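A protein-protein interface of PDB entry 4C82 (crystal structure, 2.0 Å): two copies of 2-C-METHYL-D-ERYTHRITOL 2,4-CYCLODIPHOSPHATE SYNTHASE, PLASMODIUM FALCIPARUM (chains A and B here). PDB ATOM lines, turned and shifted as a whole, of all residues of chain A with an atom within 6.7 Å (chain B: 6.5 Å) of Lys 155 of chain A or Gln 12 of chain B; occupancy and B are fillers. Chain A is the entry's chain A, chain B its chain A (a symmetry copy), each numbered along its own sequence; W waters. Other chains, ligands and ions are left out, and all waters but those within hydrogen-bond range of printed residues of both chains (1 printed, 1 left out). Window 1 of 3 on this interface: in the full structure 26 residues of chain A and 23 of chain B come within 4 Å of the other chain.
OE1 of Gln 12 of chain A lies close to OE1 of Gln 12 of chain B (2.8 Å).
OD2 of Asp 120 of chain A lies within hydrogen-bond range of N of Gln 12 of chain B (2.8 Å).
ND2 of Asn 122 of chain A is in hydrogen-bond range of O of Gln 12 of chain B (2.8 Å).
The guanidinium group (NH2) of Arg 134 of chain A lies within salt-bridge range of the side-chain carboxylate (OD2) of Asp 81 of chain B (3.0 Å).
O of Gln 12 of chain B sits at hydrogen-bond distance from NZ of Lys 155 of chain A, 3.1 Å away.
The side-chain amide nitrogen (ND2) of Asn 176 of chain A sits close to the side-chain amide nitrogen (NE2) of Gln 12 of chain B.
The side-chain hydroxyl (OG) of Ser 153 of chain A lies within hydrogen-bond range of the side-chain carboxylate (OD1) of Asp 120 of chain A (2.8 Å).
The side-chain carboxylate (OD1) of Asp 120 of chain A lies within salt-bridge range of the side-chain amino group (NZ) of Lys 155 of chain A, at 2.6 Å.
The backbone carbonyl oxygen (O) of Asp 120 of chain A lies within hydrogen-bond range of the backbone NH (N) of Asn 176 of chain A (2.7 Å).
The backbone carbonyl oxygen of Ile 121 of chain A lies within hydrogen-bond range of the backbone NH of Lys 155 of chain A (2.8 Å).
N of Gly 11 of chain B lies within hydrogen-bond range of O of Ile 177 of chain B (3.0 Å).
The backbone carbonyl oxygen (O) of Leu 74 of chain B lies within hydrogen-bond range of the backbone NH (N) of Ser 79 of chain B, 3.0 Å away.
Among the printed residues, merely in contact across the chains: Asp 120 of chain A with Ile 10 of chain B (3.96 Å), Asp 120 of chain A with Gly 11 of chain B (3.4 Å), Asp 120 of chain A with Gly 75 of chain B (3.4 Å), Asp 120 of chain A with Ala 76 of chain B (3.97 Å), Ile 124 of chain A with Tyr 14 of chain B (3.9 Å), Arg 134 of chain A with Ser 79 of chain B (3.8 Å), Ser 153 of chain A with Gly 75 of chain B (3.2 Å), Lys 155 of chain A with Asp 71 of chain B (3.3 Å), Lys 157 of chain A with Tyr 14 of chain B (3.7 Å), Phe 174 of chain A with Gln 12 of chain B (3.5 Å), Phe 174 of chain A with Phe 174 of chain B (3.9 Å) and Asn 176 of chain A with Ile 10 of chain B (3.9 Å).
Of chain B, only Gln 12 (3.1 Å) and Asp 71 (3.3 Å) come within 4 Å of Lys 155 of chain A.
Gln 12 of chain B touches just these residues of chain A: Gln 12, Asp 120, Asn 122, Lys 155, Phe 174 and Asn 176.
Printed residues of chain B within 4 Å of Ser 153 of chain A: Gly 75.
Printed residues of chain A within 4 Å of Asp 81 of chain B: Arg 134.
Of the printed residues of chain B, Arg 134 of chain A touches Ser 79 and Asp 81.
Printed residues of chain B within 4 Å of Asp 120 of chain A: Ile 10, Gly 11, Gln 12, Gly 75 and Ala 76.
Printed residues of chain B within 4 Å of Lys 157 of chain A: Tyr 14.
Ile 73 of chain B touches none of the printed residues of chain A.
The nearest printed residue of chain B that does not touch Asn 176 of chain A is Asn 176 of chain B (4.6 Å).
Printed residues of chain B that touch a printed residue of chain A: Ile 10, Gly 11, Gln 12, Tyr 14, Asp 71, Gly 75, Ala 76, Ser 79, Asp 81 and Phe 174.
Hydrophobic or aromatic side chains of chain B within 4 Å of the printed part of chain A: Ile 10, Tyr 14 and Phe 174.
Hydrophobic or aromatic side chains of chain A that line the printed part of chain B: Ile 124 and Phe 174.
Along chain A the printed residues that touch a printed residue of chain B span positions 12 to 176.
Among the printed residues, 18 pairs touch across the chains.
Gln 12 of chain A touches its own counterpart, Gln 12 of chain B.
Phe 174 of chain A touches Gln 12 of chain B, but with the chains exchanged Gln 12 of chain A does not touch Phe 174 of chain B (5.9 Å).
Phe 174 of chain A touches its own counterpart, Phe 174 of chain B.
Asn 176 of chain A touches Gln 12 of chain B, but with the chains exchanged Gln 12 of chain A does not touch Asn 176 of chain B (4.8 Å).
Water W1 lies within hydrogen-bond range of N of Gly 156 of chain A (2.7 Å), OD2 of Asp 81 of chain B (2.7 Å) and NH1 of Arg 134 of chain A (3.2 Å).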
ATOM      1  N   GLN A  12      -8.988 -14.105   4.650  1.00  0.00           N
ATOM      2  CA  GLN A  12     -10.434 -14.265   4.646  1.00  0.00           C
ATOM      3  C   GLN A  12     -10.749 -15.753   4.541  1.00  0.00           C
ATOM      4  O   GLN A  12     -10.321 -16.380   3.576  1.00  0.00           O
ATOM      5  CB  GLN A  12     -11.020 -13.444   3.511  1.00  0.00           C
ATOM      6  CG  GLN A  12     -12.543 -13.656   3.432  1.00  0.00           C
ATOM      7  CD  GLN A  12     -13.162 -12.939   2.308  1.00  0.00           C
ATOM      8  OE1 GLN A  12     -13.760 -11.856   2.490  1.00  0.00           O
ATOM      9  NE2 GLN A  12     -13.002 -13.497   1.104  1.00  0.00           N
ATOM     10  N   GLY A  13     -11.449 -16.324   5.500  1.00  0.00           N
ATOM     11  CA  GLY A  13     -11.796 -17.741   5.331  1.00  0.00           C
ATOM     12  C   GLY A  13     -13.251 -17.825   4.778  1.00  0.00           C
ATOM     13  O   GLY A  13     -14.098 -16.936   5.010  1.00  0.00           O
ATOM     14  N   ASP A 120     -13.494 -10.817  12.335  1.00  0.00           N
ATOM     15  CA  ASP A 120     -14.897 -10.464  12.135  1.00  0.00           C
ATOM     16  C   ASP A 120     -15.477 -11.620  11.248  1.00  0.00           C
ATOM     17  O   ASP A 120     -14.932 -11.909  10.213  1.00  0.00           O
ATOM     18  CB  ASP A 120     -14.998  -9.114  11.502  1.00  0.00           C
ATOM     19  CG  ASP A 120     -16.461  -8.604  11.414  1.00  0.00           C
ATOM     20  OD1 ASP A 120     -17.351  -9.119  12.147  1.00  0.00           O
ATOM     21  OD2 ASP A 120     -16.684  -7.696  10.610  1.00  0.00           O
ATOM     22  N   ILE A 121     -16.482 -12.288  11.775  1.00  0.00           N
ATOM     23  CA  ILE A 121     -17.168 -13.479  11.236  1.00  0.00           C
ATOM     24  C   ILE A 121     -18.639 -13.164  10.842  1.00  0.00           C
ATOM     25  O   ILE A 121     -19.398 -12.671  11.642  1.00  0.00           O
ATOM     26  CB  ILE A 121     -17.132 -14.555  12.359  1.00  0.00           C
ATOM     27  CG1 ILE A 121     -15.641 -14.816  12.749  1.00  0.00           C
ATOM     28  CG2 ILE A 121     -17.750 -15.874  11.891  1.00  0.00           C
ATOM     29  CD1 ILE A 121     -15.368 -15.386  14.141  1.00  0.00           C
ATOM     30  N   ASN A 122     -19.030 -13.497   9.620  1.00  0.00           N
ATOM     31  CA  ASN A 122     -20.368 -13.257   9.096  1.00  0.00           C
ATOM     32  C   ASN A 122     -20.889 -14.627   8.783  1.00  0.00           C
ATOM     33  O   ASN A 122     -20.395 -15.276   7.828  1.00  0.00           O
ATOM     34  CB  ASN A 122     -20.248 -12.474   7.743  1.00  0.00           C
ATOM     35  CG  ASN A 122     -20.063 -10.974   7.956  1.00  0.00           C
ATOM     36  OD1 ASN A 122     -20.777 -10.405   8.749  1.00  0.00           O
ATOM     37  ND2 ASN A 122     -19.122 -10.339   7.260  1.00  0.00           N
ATOM     38  N   VAL A 123     -21.842 -15.090   9.570  1.00  0.00           N
ATOM     39  CA  VAL A 123     -22.489 -16.387   9.271  1.00  0.00           C
ATOM     40  C   VAL A 123     -23.737 -16.028   8.416  1.00  0.00           C
ATOM     41  O   VAL A 123     -24.549 -15.145   8.801  1.00  0.00           O
ATOM     42  CB  VAL A 123     -22.899 -17.021  10.607  1.00  0.00           C
ATOM     43  CG1 VAL A 123     -23.599 -18.371  10.421  1.00  0.00           C
ATOM     44  CG2 VAL A 123     -21.696 -17.087  11.546  1.00  0.00           C
ATOM     45  N   ILE A 124     -23.878 -16.665   7.251  1.00  0.00           N
ATOM     46  CA  ILE A 124     -25.008 -16.367   6.352  1.00  0.00           C
ATOM     47  C   ILE A 124     -25.821 -17.664   6.373  1.00  0.00           C
ATOM     48  O   ILE A 124     -25.411 -18.734   5.820  1.00  0.00           O
ATOM     49  CB  ILE A 124     -24.530 -16.005   4.927  1.00  0.00           C
ATOM     50  CG1 ILE A 124     -23.424 -14.892   5.027  1.00  0.00           C
ATOM     51  CG2 ILE A 124     -25.746 -15.573   4.052  1.00  0.00           C
ATOM     52  CD1 ILE A 124     -22.853 -14.336   3.681  1.00  0.00           C
ATOM     53  N   ILE A 130     -28.280 -16.430  15.038  1.00  0.00           N
ATOM     54  CA  ILE A 130     -26.951 -16.415  15.677  1.00  0.00           C
ATOM     55  C   ILE A 130     -26.969 -15.604  16.987  1.00  0.00           C
ATOM     56  O   ILE A 130     -26.243 -15.931  17.933  1.00  0.00           O
ATOM     57  CB  ILE A 130     -25.842 -15.901  14.691  1.00  0.00           C
ATOM     58  CG1 ILE A 130     -25.777 -16.733  13.385  1.00  0.00           C
ATOM     59  CG2 ILE A 130     -24.446 -15.819  15.317  1.00  0.00           C
ATOM     60  CD1 ILE A 130     -25.783 -18.259  13.511  1.00  0.00           C
ATOM     61  N   ARG A 134     -24.591 -16.203  20.301  1.00  0.00           N
ATOM     62  CA  ARG A 134     -23.419 -15.383  19.969  1.00  0.00           C
ATOM     63  C   ARG A 134     -22.411 -15.282  21.137  1.00  0.00           C
ATOM     64  O   ARG A 134     -21.167 -15.471  20.947  1.00  0.00           O
ATOM     65  CB  ARG A 134     -23.900 -13.983  19.609  1.00  0.00           C
ATOM     66  CG  ARG A 134     -22.799 -13.018  19.270  1.00  0.00           C
ATOM     67  CD  ARG A 134     -23.238 -11.609  19.600  1.00  0.00           C
ATOM     68  NE  ARG A 134     -22.862 -10.687  18.554  1.00  0.00           N
ATOM     69  CZ  ARG A 134     -23.678 -10.362  17.540  1.00  0.00           C
ATOM     70  NH1 ARG A 134     -24.897 -10.905  17.481  1.00  0.00           N
ATOM     71  NH2 ARG A 134     -23.283  -9.506  16.581  1.00  0.00           N
ATOM     72  N   SER A 153     -15.784 -10.738  16.733  1.00  0.00           N
ATOM     73  CA  SER A 153     -17.142 -10.256  16.402  1.00  0.00           C
ATOM     74  C   SER A 153     -17.770 -11.439  15.671  1.00  0.00           C
ATOM     75  O   SER A 153     -17.080 -12.030  14.822  1.00  0.00           O
ATOM     76  CB  SER A 153     -17.055  -9.124  15.431  1.00  0.00           C
ATOM     77  OG  SER A 153     -18.329  -8.977  14.762  1.00  0.00           O
ATOM     78  N   VAL A 154     -18.993 -11.837  16.026  1.00  0.00           N
ATOM     79  CA  VAL A 154     -19.633 -12.903  15.269  1.00  0.00           C
ATOM     80  C   VAL A 154     -21.035 -12.352  14.939  1.00  0.00           C
ATOM     81  O   VAL A 154     -21.747 -11.964  15.871  1.00  0.00           O
ATOM     82  CB  VAL A 154     -19.758 -14.255  16.028  1.00  0.00           C
ATOM     83  CG1 VAL A 154     -18.441 -14.866  16.419  1.00  0.00           C
ATOM     84  CG2 VAL A 154     -20.592 -14.120  17.263  1.00  0.00           C
ATOM     85  N   LYS A 155     -21.398 -12.280  13.634  1.00  0.00           N
ATOM     86  CA  LYS A 155     -22.653 -11.689  13.187  1.00  0.00           C
ATOM     87  C   LYS A 155     -23.424 -12.676  12.308  1.00  0.00           C
ATOM     88  O   LYS A 155     -22.804 -13.419  11.534  1.00  0.00           O
ATOM     89  CB  LYS A 155     -22.465 -10.394  12.392  1.00  0.00           C
ATOM     90  CG  LYS A 155     -21.330  -9.487  12.842  1.00  0.00           C
ATOM     91  CD  LYS A 155     -21.390  -8.086  12.241  1.00  0.00           C
ATOM     92  CE  LYS A 155     -20.676  -7.963  10.897  1.00  0.00           C
ATOM     93  NZ  LYS A 155     -19.419  -8.717  10.683  1.00  0.00           N
ATOM     94  N   GLY A 156     -24.762 -12.664  12.403  1.00  0.00           N
ATOM     95  CA  GLY A 156     -25.579 -13.669  11.657  1.00  0.00           C
ATOM     96  C   GLY A 156     -26.412 -12.883  10.665  1.00  0.00           C
ATOM     97  O   GLY A 156     -26.847 -11.795  10.981  1.00  0.00           O
ATOM     98  N   LYS A 157     -26.554 -13.379   9.436  1.00  0.00           N
ATOM     99  CA  LYS A 157     -27.376 -12.686   8.484  1.00  0.00           C
ATOM    100  C   LYS A 157     -28.216 -13.714   7.860  1.00  0.00           C
ATOM    101  O   LYS A 157     -27.686 -14.698   7.401  1.00  0.00           O
ATOM    102  CB  LYS A 157     -26.512 -12.034   7.394  1.00  0.00           C
ATOM    103  CG  LYS A 157     -25.967 -10.631   7.828  1.00  0.00           C
ATOM    104  CD  LYS A 157     -27.113  -9.589   7.881  1.00  0.00           C
ATOM    105  CE  LYS A 157     -28.067  -9.712   6.662  1.00  0.00           C
ATOM    106  NZ  LYS A 157     -29.065  -8.599   6.545  1.00  0.00           N
ATOM    107  N   PHE A 174     -18.141 -16.356   6.385  1.00  0.00           N
ATOM    108  CA  PHE A 174     -16.936 -15.615   5.966  1.00  0.00           C
ATOM    109  C   PHE A 174     -16.231 -15.162   7.260  1.00  0.00           C
ATOM    110  O   PHE A 174     -16.873 -14.675   8.156  1.00  0.00           O
ATOM    111  CB  PHE A 174     -17.292 -14.372   5.186  1.00  0.00           C
ATOM    112  CG  PHE A 174     -17.707 -14.619   3.738  1.00  0.00           C
ATOM    113  CD1 PHE A 174     -19.012 -14.890   3.449  1.00  0.00           C
ATOM    114  CD2 PHE A 174     -16.795 -14.602   2.683  1.00  0.00           C
ATOM    115  CE1 PHE A 174     -19.429 -15.133   2.144  1.00  0.00           C
ATOM    116  CE2 PHE A 174     -17.209 -14.818   1.348  1.00  0.00           C
ATOM    117  CZ  PHE A 174     -18.531 -15.087   1.080  1.00  0.00           C
ATOM    118  N   ALA A 175     -14.939 -15.380   7.367  1.00  0.00           N
ATOM    119  CA  ALA A 175     -14.245 -14.970   8.543  1.00  0.00           C
ATOM    120  C   ALA A 175     -13.064 -14.053   8.088  1.00  0.00           C
ATOM    121  O   ALA A 175     -12.297 -14.413   7.241  1.00  0.00           O
ATOM    122  CB  ALA A 175     -13.738 -16.218   9.299  1.00  0.00           C
ATOM    123  N   ASN A 176     -12.960 -12.867   8.666  1.00  0.00           N
ATOM    124  CA  ASN A 176     -11.968 -11.896   8.199  1.00  0.00           C
ATOM    125  C   ASN A 176     -11.065 -11.601   9.392  1.00  0.00           C
ATOM    126  O   ASN A 176     -11.540 -11.323  10.481  1.00  0.00           O
ATOM    127  CB  ASN A 176     -12.653 -10.605   7.764  1.00  0.00           C
ATOM    128  CG  ASN A 176     -13.713 -10.879   6.663  1.00  0.00           C
ATOM    129  OD1 ASN A 176     -13.430 -10.740   5.491  1.00  0.00           O
ATOM    130  ND2 ASN A 176     -14.867 -11.369   7.059  1.00  0.00           N
ATOM    131  N   ILE B  10     -10.034  -4.861  11.376  1.00  0.00           N
ATOM    132  CA  ILE B  10     -10.726  -5.174  10.152  1.00  0.00           C
ATOM    133  C   ILE B  10     -12.214  -5.386  10.446  1.00  0.00           C
ATOM    134  O   ILE B  10     -12.619  -5.953  11.534  1.00  0.00           O
ATOM    135  CB  ILE B  10     -10.081  -6.370   9.378  1.00  0.00           C
ATOM    136  CG1 ILE B  10     -10.766  -6.623   8.020  1.00  0.00           C
ATOM    137  CG2 ILE B  10     -10.080  -7.739  10.184  1.00  0.00           C
ATOM    138  CD1 ILE B  10     -10.067  -7.773   7.270  1.00  0.00           C
ATOM    139  N   GLY B  11     -13.045  -4.974   9.462  1.00  0.00           N
ATOM    140  CA  GLY B  11     -14.519  -5.284   9.562  1.00  0.00           C
ATOM    141  C   GLY B  11     -15.008  -5.724   8.168  1.00  0.00           C
ATOM    142  O   GLY B  11     -14.561  -5.199   7.159  1.00  0.00           O
ATOM    143  N   GLN B  12     -15.955  -6.665   8.124  1.00  0.00           N
ATOM    144  CA  GLN B  12     -16.599  -6.906   6.841  1.00  0.00           C
ATOM    145  C   GLN B  12     -18.108  -6.871   7.052  1.00  0.00           C
ATOM    146  O   GLN B  12     -18.611  -7.655   7.853  1.00  0.00           O
ATOM    147  CB  GLN B  12     -16.101  -8.224   6.276  1.00  0.00           C
ATOM    148  CG  GLN B  12     -16.825  -8.545   4.957  1.00  0.00           C
ATOM    149  CD  GLN B  12     -16.434  -9.845   4.392  1.00  0.00           C
ATOM    150  OE1 GLN B  12     -15.611  -9.915   3.453  1.00  0.00           O
ATOM    151  NE2 GLN B  12     -16.978 -10.918   4.974  1.00  0.00           N
ATOM    152  N   GLY B  13     -18.823  -5.986   6.387  1.00  0.00           N
ATOM    153  CA  GLY B  13     -20.281  -6.029   6.559  1.00  0.00           C
ATOM    154  C   GLY B  13     -20.892  -6.816   5.360  1.00  0.00           C
ATOM    155  O   GLY B  13     -20.333  -6.856   4.243  1.00  0.00           O
ATOM    156  N   TYR B  14     -22.006  -7.459   5.598  1.00  0.00           N
ATOM    157  CA  TYR B  14     -22.710  -8.086   4.476  1.00  0.00           C
ATOM    158  C   TYR B  14     -24.193  -7.779   4.595  1.00  0.00           C
ATOM    159  O   TYR B  14     -24.754  -7.761   5.719  1.00  0.00           O
ATOM    160  CB  TYR B  14     -22.465  -9.622   4.561  1.00  0.00           C
ATOM    161  CG  TYR B  14     -23.403 -10.362   3.621  1.00  0.00           C
ATOM    162  CD1 TYR B  14     -23.076 -10.524   2.322  1.00  0.00           C
ATOM    163  CD2 TYR B  14     -24.648 -10.839   4.061  1.00  0.00           C
ATOM    164  CE1 TYR B  14     -23.904 -11.229   1.448  1.00  0.00           C
ATOM    165  CE2 TYR B  14     -25.516 -11.523   3.199  1.00  0.00           C
ATOM    166  CZ  TYR B  14     -25.126 -11.728   1.892  1.00  0.00           C
ATOM    167  OH  TYR B  14     -25.966 -12.380   0.935  1.00  0.00           O
ATOM    168  N   SER B  68     -24.550  -2.327   5.111  1.00  0.00           N
ATOM    169  CA  SER B  68     -23.372  -3.219   5.244  1.00  0.00           C
ATOM    170  C   SER B  68     -22.229  -2.376   5.794  1.00  0.00           C
ATOM    171  O   SER B  68     -21.382  -2.863   6.544  1.00  0.00           O
ATOM    172  CB  SER B  68     -22.971  -3.918   3.923  1.00  0.00           C
ATOM    173  OG  SER B  68     -22.618  -2.977   2.996  1.00  0.00           O
ATOM    174  N   ASP B  71     -22.576  -2.458   9.413  1.00  0.00           N
ATOM    175  CA  ASP B  71     -22.210  -3.752   9.944  1.00  0.00           C
ATOM    176  C   ASP B  71     -20.708  -3.982   9.912  1.00  0.00           C
ATOM    177  O   ASP B  71     -20.216  -4.702  10.771  1.00  0.00           O
ATOM    178  CB  ASP B  71     -22.962  -4.879   9.209  1.00  0.00           C
ATOM    179  CG  ASP B  71     -24.255  -5.268   9.919  1.00  0.00           C
ATOM    180  OD1 ASP B  71     -24.651  -4.586  10.911  1.00  0.00           O
ATOM    181  OD2 ASP B  71     -24.864  -6.273   9.510  1.00  0.00           O
ATOM    182  N   SER B  72     -19.990  -3.388   8.950  1.00  0.00           N
ATOM    183  CA  SER B  72     -18.525  -3.563   8.903  1.00  0.00           C
ATOM    184  C   SER B  72     -17.844  -2.806  10.107  1.00  0.00           C
ATOM    185  O   SER B  72     -16.816  -3.272  10.667  1.00  0.00           O
ATOM    186  CB  SER B  72     -17.880  -3.092   7.599  1.00  0.00           C
ATOM    187  OG  SER B  72     -17.879  -1.706   7.406  1.00  0.00           O
ATOM    188  N   ILE B  73     -18.424  -1.661  10.440  1.00  0.00           N
ATOM    189  CA  ILE B  73     -17.937  -0.862  11.604  1.00  0.00           C
ATOM    190  C   ILE B  73     -18.187  -1.582  12.887  1.00  0.00           C
ATOM    191  O   ILE B  73     -17.258  -1.754  13.676  1.00  0.00           O
ATOM    192  CB  ILE B  73     -18.566   0.540  11.622  1.00  0.00           C
ATOM    193  CG1 ILE B  73     -17.972   1.313  10.451  1.00  0.00           C
ATOM    194  CG2 ILE B  73     -18.302   1.266  13.001  1.00  0.00           C
ATOM    195  CD1 ILE B  73     -18.785   2.497   9.863  1.00  0.00           C
ATOM    196  N   LEU B  74     -19.419  -2.105  13.057  1.00  0.00           N
ATOM    197  CA  LEU B  74     -19.767  -2.822  14.245  1.00  0.00           C
ATOM    198  C   LEU B  74     -18.960  -4.044  14.354  1.00  0.00           C
ATOM    199  O   LEU B  74     -18.485  -4.397  15.452  1.00  0.00           O
ATOM    200  CB  LEU B  74     -21.268  -3.244  14.225  1.00  0.00           C
ATOM    201  CG  LEU B  74     -22.308  -2.254  14.859  1.00  0.00           C
ATOM    202  CD1 LEU B  74     -21.821  -0.818  14.910  1.00  0.00           C
ATOM    203  CD2 LEU B  74     -23.716  -2.399  14.269  1.00  0.00           C
ATOM    204  N   GLY B  75     -18.768  -4.718  13.206  1.00  0.00           N
ATOM    205  CA  GLY B  75     -17.983  -5.899  13.229  1.00  0.00           C
ATOM    206  C   GLY B  75     -16.527  -5.590  13.561  1.00  0.00           C
ATOM    207  O   GLY B  75     -15.883  -6.314  14.337  1.00  0.00           O
ATOM    208  N   ALA B  76     -15.970  -4.558  12.934  1.00  0.00           N
ATOM    209  CA  ALA B  76     -14.616  -4.243  13.261  1.00  0.00           C
ATOM    210  C   ALA B  76     -14.422  -4.070  14.769  1.00  0.00           C
ATOM    211  O   ALA B  76     -13.417  -4.489  15.329  1.00  0.00           O
ATOM    212  CB  ALA B  76     -14.152  -3.021  12.480  1.00  0.00           C
ATOM    213  N   SER B  79     -19.112  -4.855  18.331  1.00  0.00           N
ATOM    214  CA  SER B  79     -20.452  -4.611  18.885  1.00  0.00           C
ATOM    215  C   SER B  79     -21.525  -5.648  18.488  1.00  0.00           C
ATOM    216  O   SER B  79     -21.372  -6.348  17.502  1.00  0.00           O
ATOM    217  CB  SER B  79     -20.953  -3.237  18.447  1.00  0.00           C
ATOM    218  OG  SER B  79     -19.934  -2.321  18.752  1.00  0.00           O
ATOM    219  N   ASP B  81     -24.973  -6.292  16.672  1.00  0.00           N
ATOM    220  CA  ASP B  81     -25.356  -5.599  15.419  1.00  0.00           C
ATOM    221  C   ASP B  81     -26.601  -4.711  15.594  1.00  0.00           C
ATOM    222  O   ASP B  81     -27.124  -4.555  16.712  1.00  0.00           O
ATOM    223  CB  ASP B  81     -25.450  -6.554  14.209  1.00  0.00           C
ATOM    224  CG  ASP B  81     -26.204  -7.823  14.530  1.00  0.00           C
ATOM    225  OD1 ASP B  81     -27.453  -7.809  14.539  1.00  0.00           O
ATOM    226  OD2 ASP B  81     -25.529  -8.838  14.785  1.00  0.00           O
ATOM    227  N   PHE B 174     -21.085  -6.311   0.035  1.00  0.00           N
ATOM    228  CA  PHE B 174     -20.004  -6.602   0.996  1.00  0.00           C
ATOM    229  C   PHE B 174     -19.256  -5.274   1.228  1.00  0.00           C
ATOM    230  O   PHE B 174     -18.964  -4.577   0.289  1.00  0.00           O
ATOM    231  CB  PHE B 174     -19.008  -7.588   0.433  1.00  0.00           C
ATOM    232  CG  PHE B 174     -19.472  -9.042   0.436  1.00  0.00           C
ATOM    233  CD1 PHE B 174     -20.190  -9.522  -0.619  1.00  0.00           C
ATOM    234  CD2 PHE B 174     -19.210  -9.911   1.496  1.00  0.00           C
ATOM    235  CE1 PHE B 174     -20.643 -10.837  -0.650  1.00  0.00           C
ATOM    236  CE2 PHE B 174     -19.638 -11.258   1.466  1.00  0.00           C
ATOM    237  CZ  PHE B 174     -20.359 -11.721   0.389  1.00  0.00           C
ATOM    238  N   ALA B 175     -19.014  -4.909   2.467  1.00  0.00           N
ATOM    239  CA  ALA B 175     -18.319  -3.692   2.727  1.00  0.00           C
ATOM    240  C   ALA B 175     -17.083  -4.046   3.618  1.00  0.00           C
ATOM    241  O   ALA B 175     -17.212  -4.688   4.620  1.00  0.00           O
ATOM    242  CB  ALA B 175     -19.268  -2.703   3.437  1.00  0.00           C
ATOM    243  N   ASN B 176     -15.899  -3.617   3.209  1.00  0.00           N
ATOM    244  CA  ASN B 176     -14.679  -4.022   3.911  1.00  0.00           C
ATOM    245  C   ASN B 176     -14.020  -2.735   4.397  1.00  0.00           C
ATOM    246  O   ASN B 176     -13.853  -1.794   3.638  1.00  0.00           O
ATOM    247  CB  ASN B 176     -13.730  -4.736   2.955  1.00  0.00           C
ATOM    248  CG  ASN B 176     -14.419  -5.963   2.298  1.00  0.00           C
ATOM    249  OD1 ASN B 176     -14.264  -7.074   2.762  1.00  0.00           O
ATOM    250  ND2 ASN B 176     -15.247  -5.719   1.307  1.00  0.00           N
ATOM    251  N   ILE B 177     -13.653  -2.737   5.668  1.00  0.00           N
ATOM    252  CA  ILE B 177     -13.188  -1.492   6.273  1.00  0.00           C
ATOM    253  C   ILE B 177     -11.966  -1.773   7.194  1.00  0.00           C
ATOM    254  O   ILE B 177     -11.812  -2.869   7.752  1.00  0.00           O
ATOM    255  CB  ILE B 177     -14.352  -0.795   7.042  1.00  0.00           C
ATOM    256  CG1 ILE B 177     -14.058   0.717   7.336  1.00  0.00           C
ATOM    257  CG2 ILE B 177     -14.673  -1.532   8.311  1.00  0.00           C
ATOM    258  CD1 ILE B 177     -15.288   1.469   7.874  1.00  0.00           C
HETATM  259  O   HOH W   1     -25.879 -11.463  14.485  1.00  0.00           O
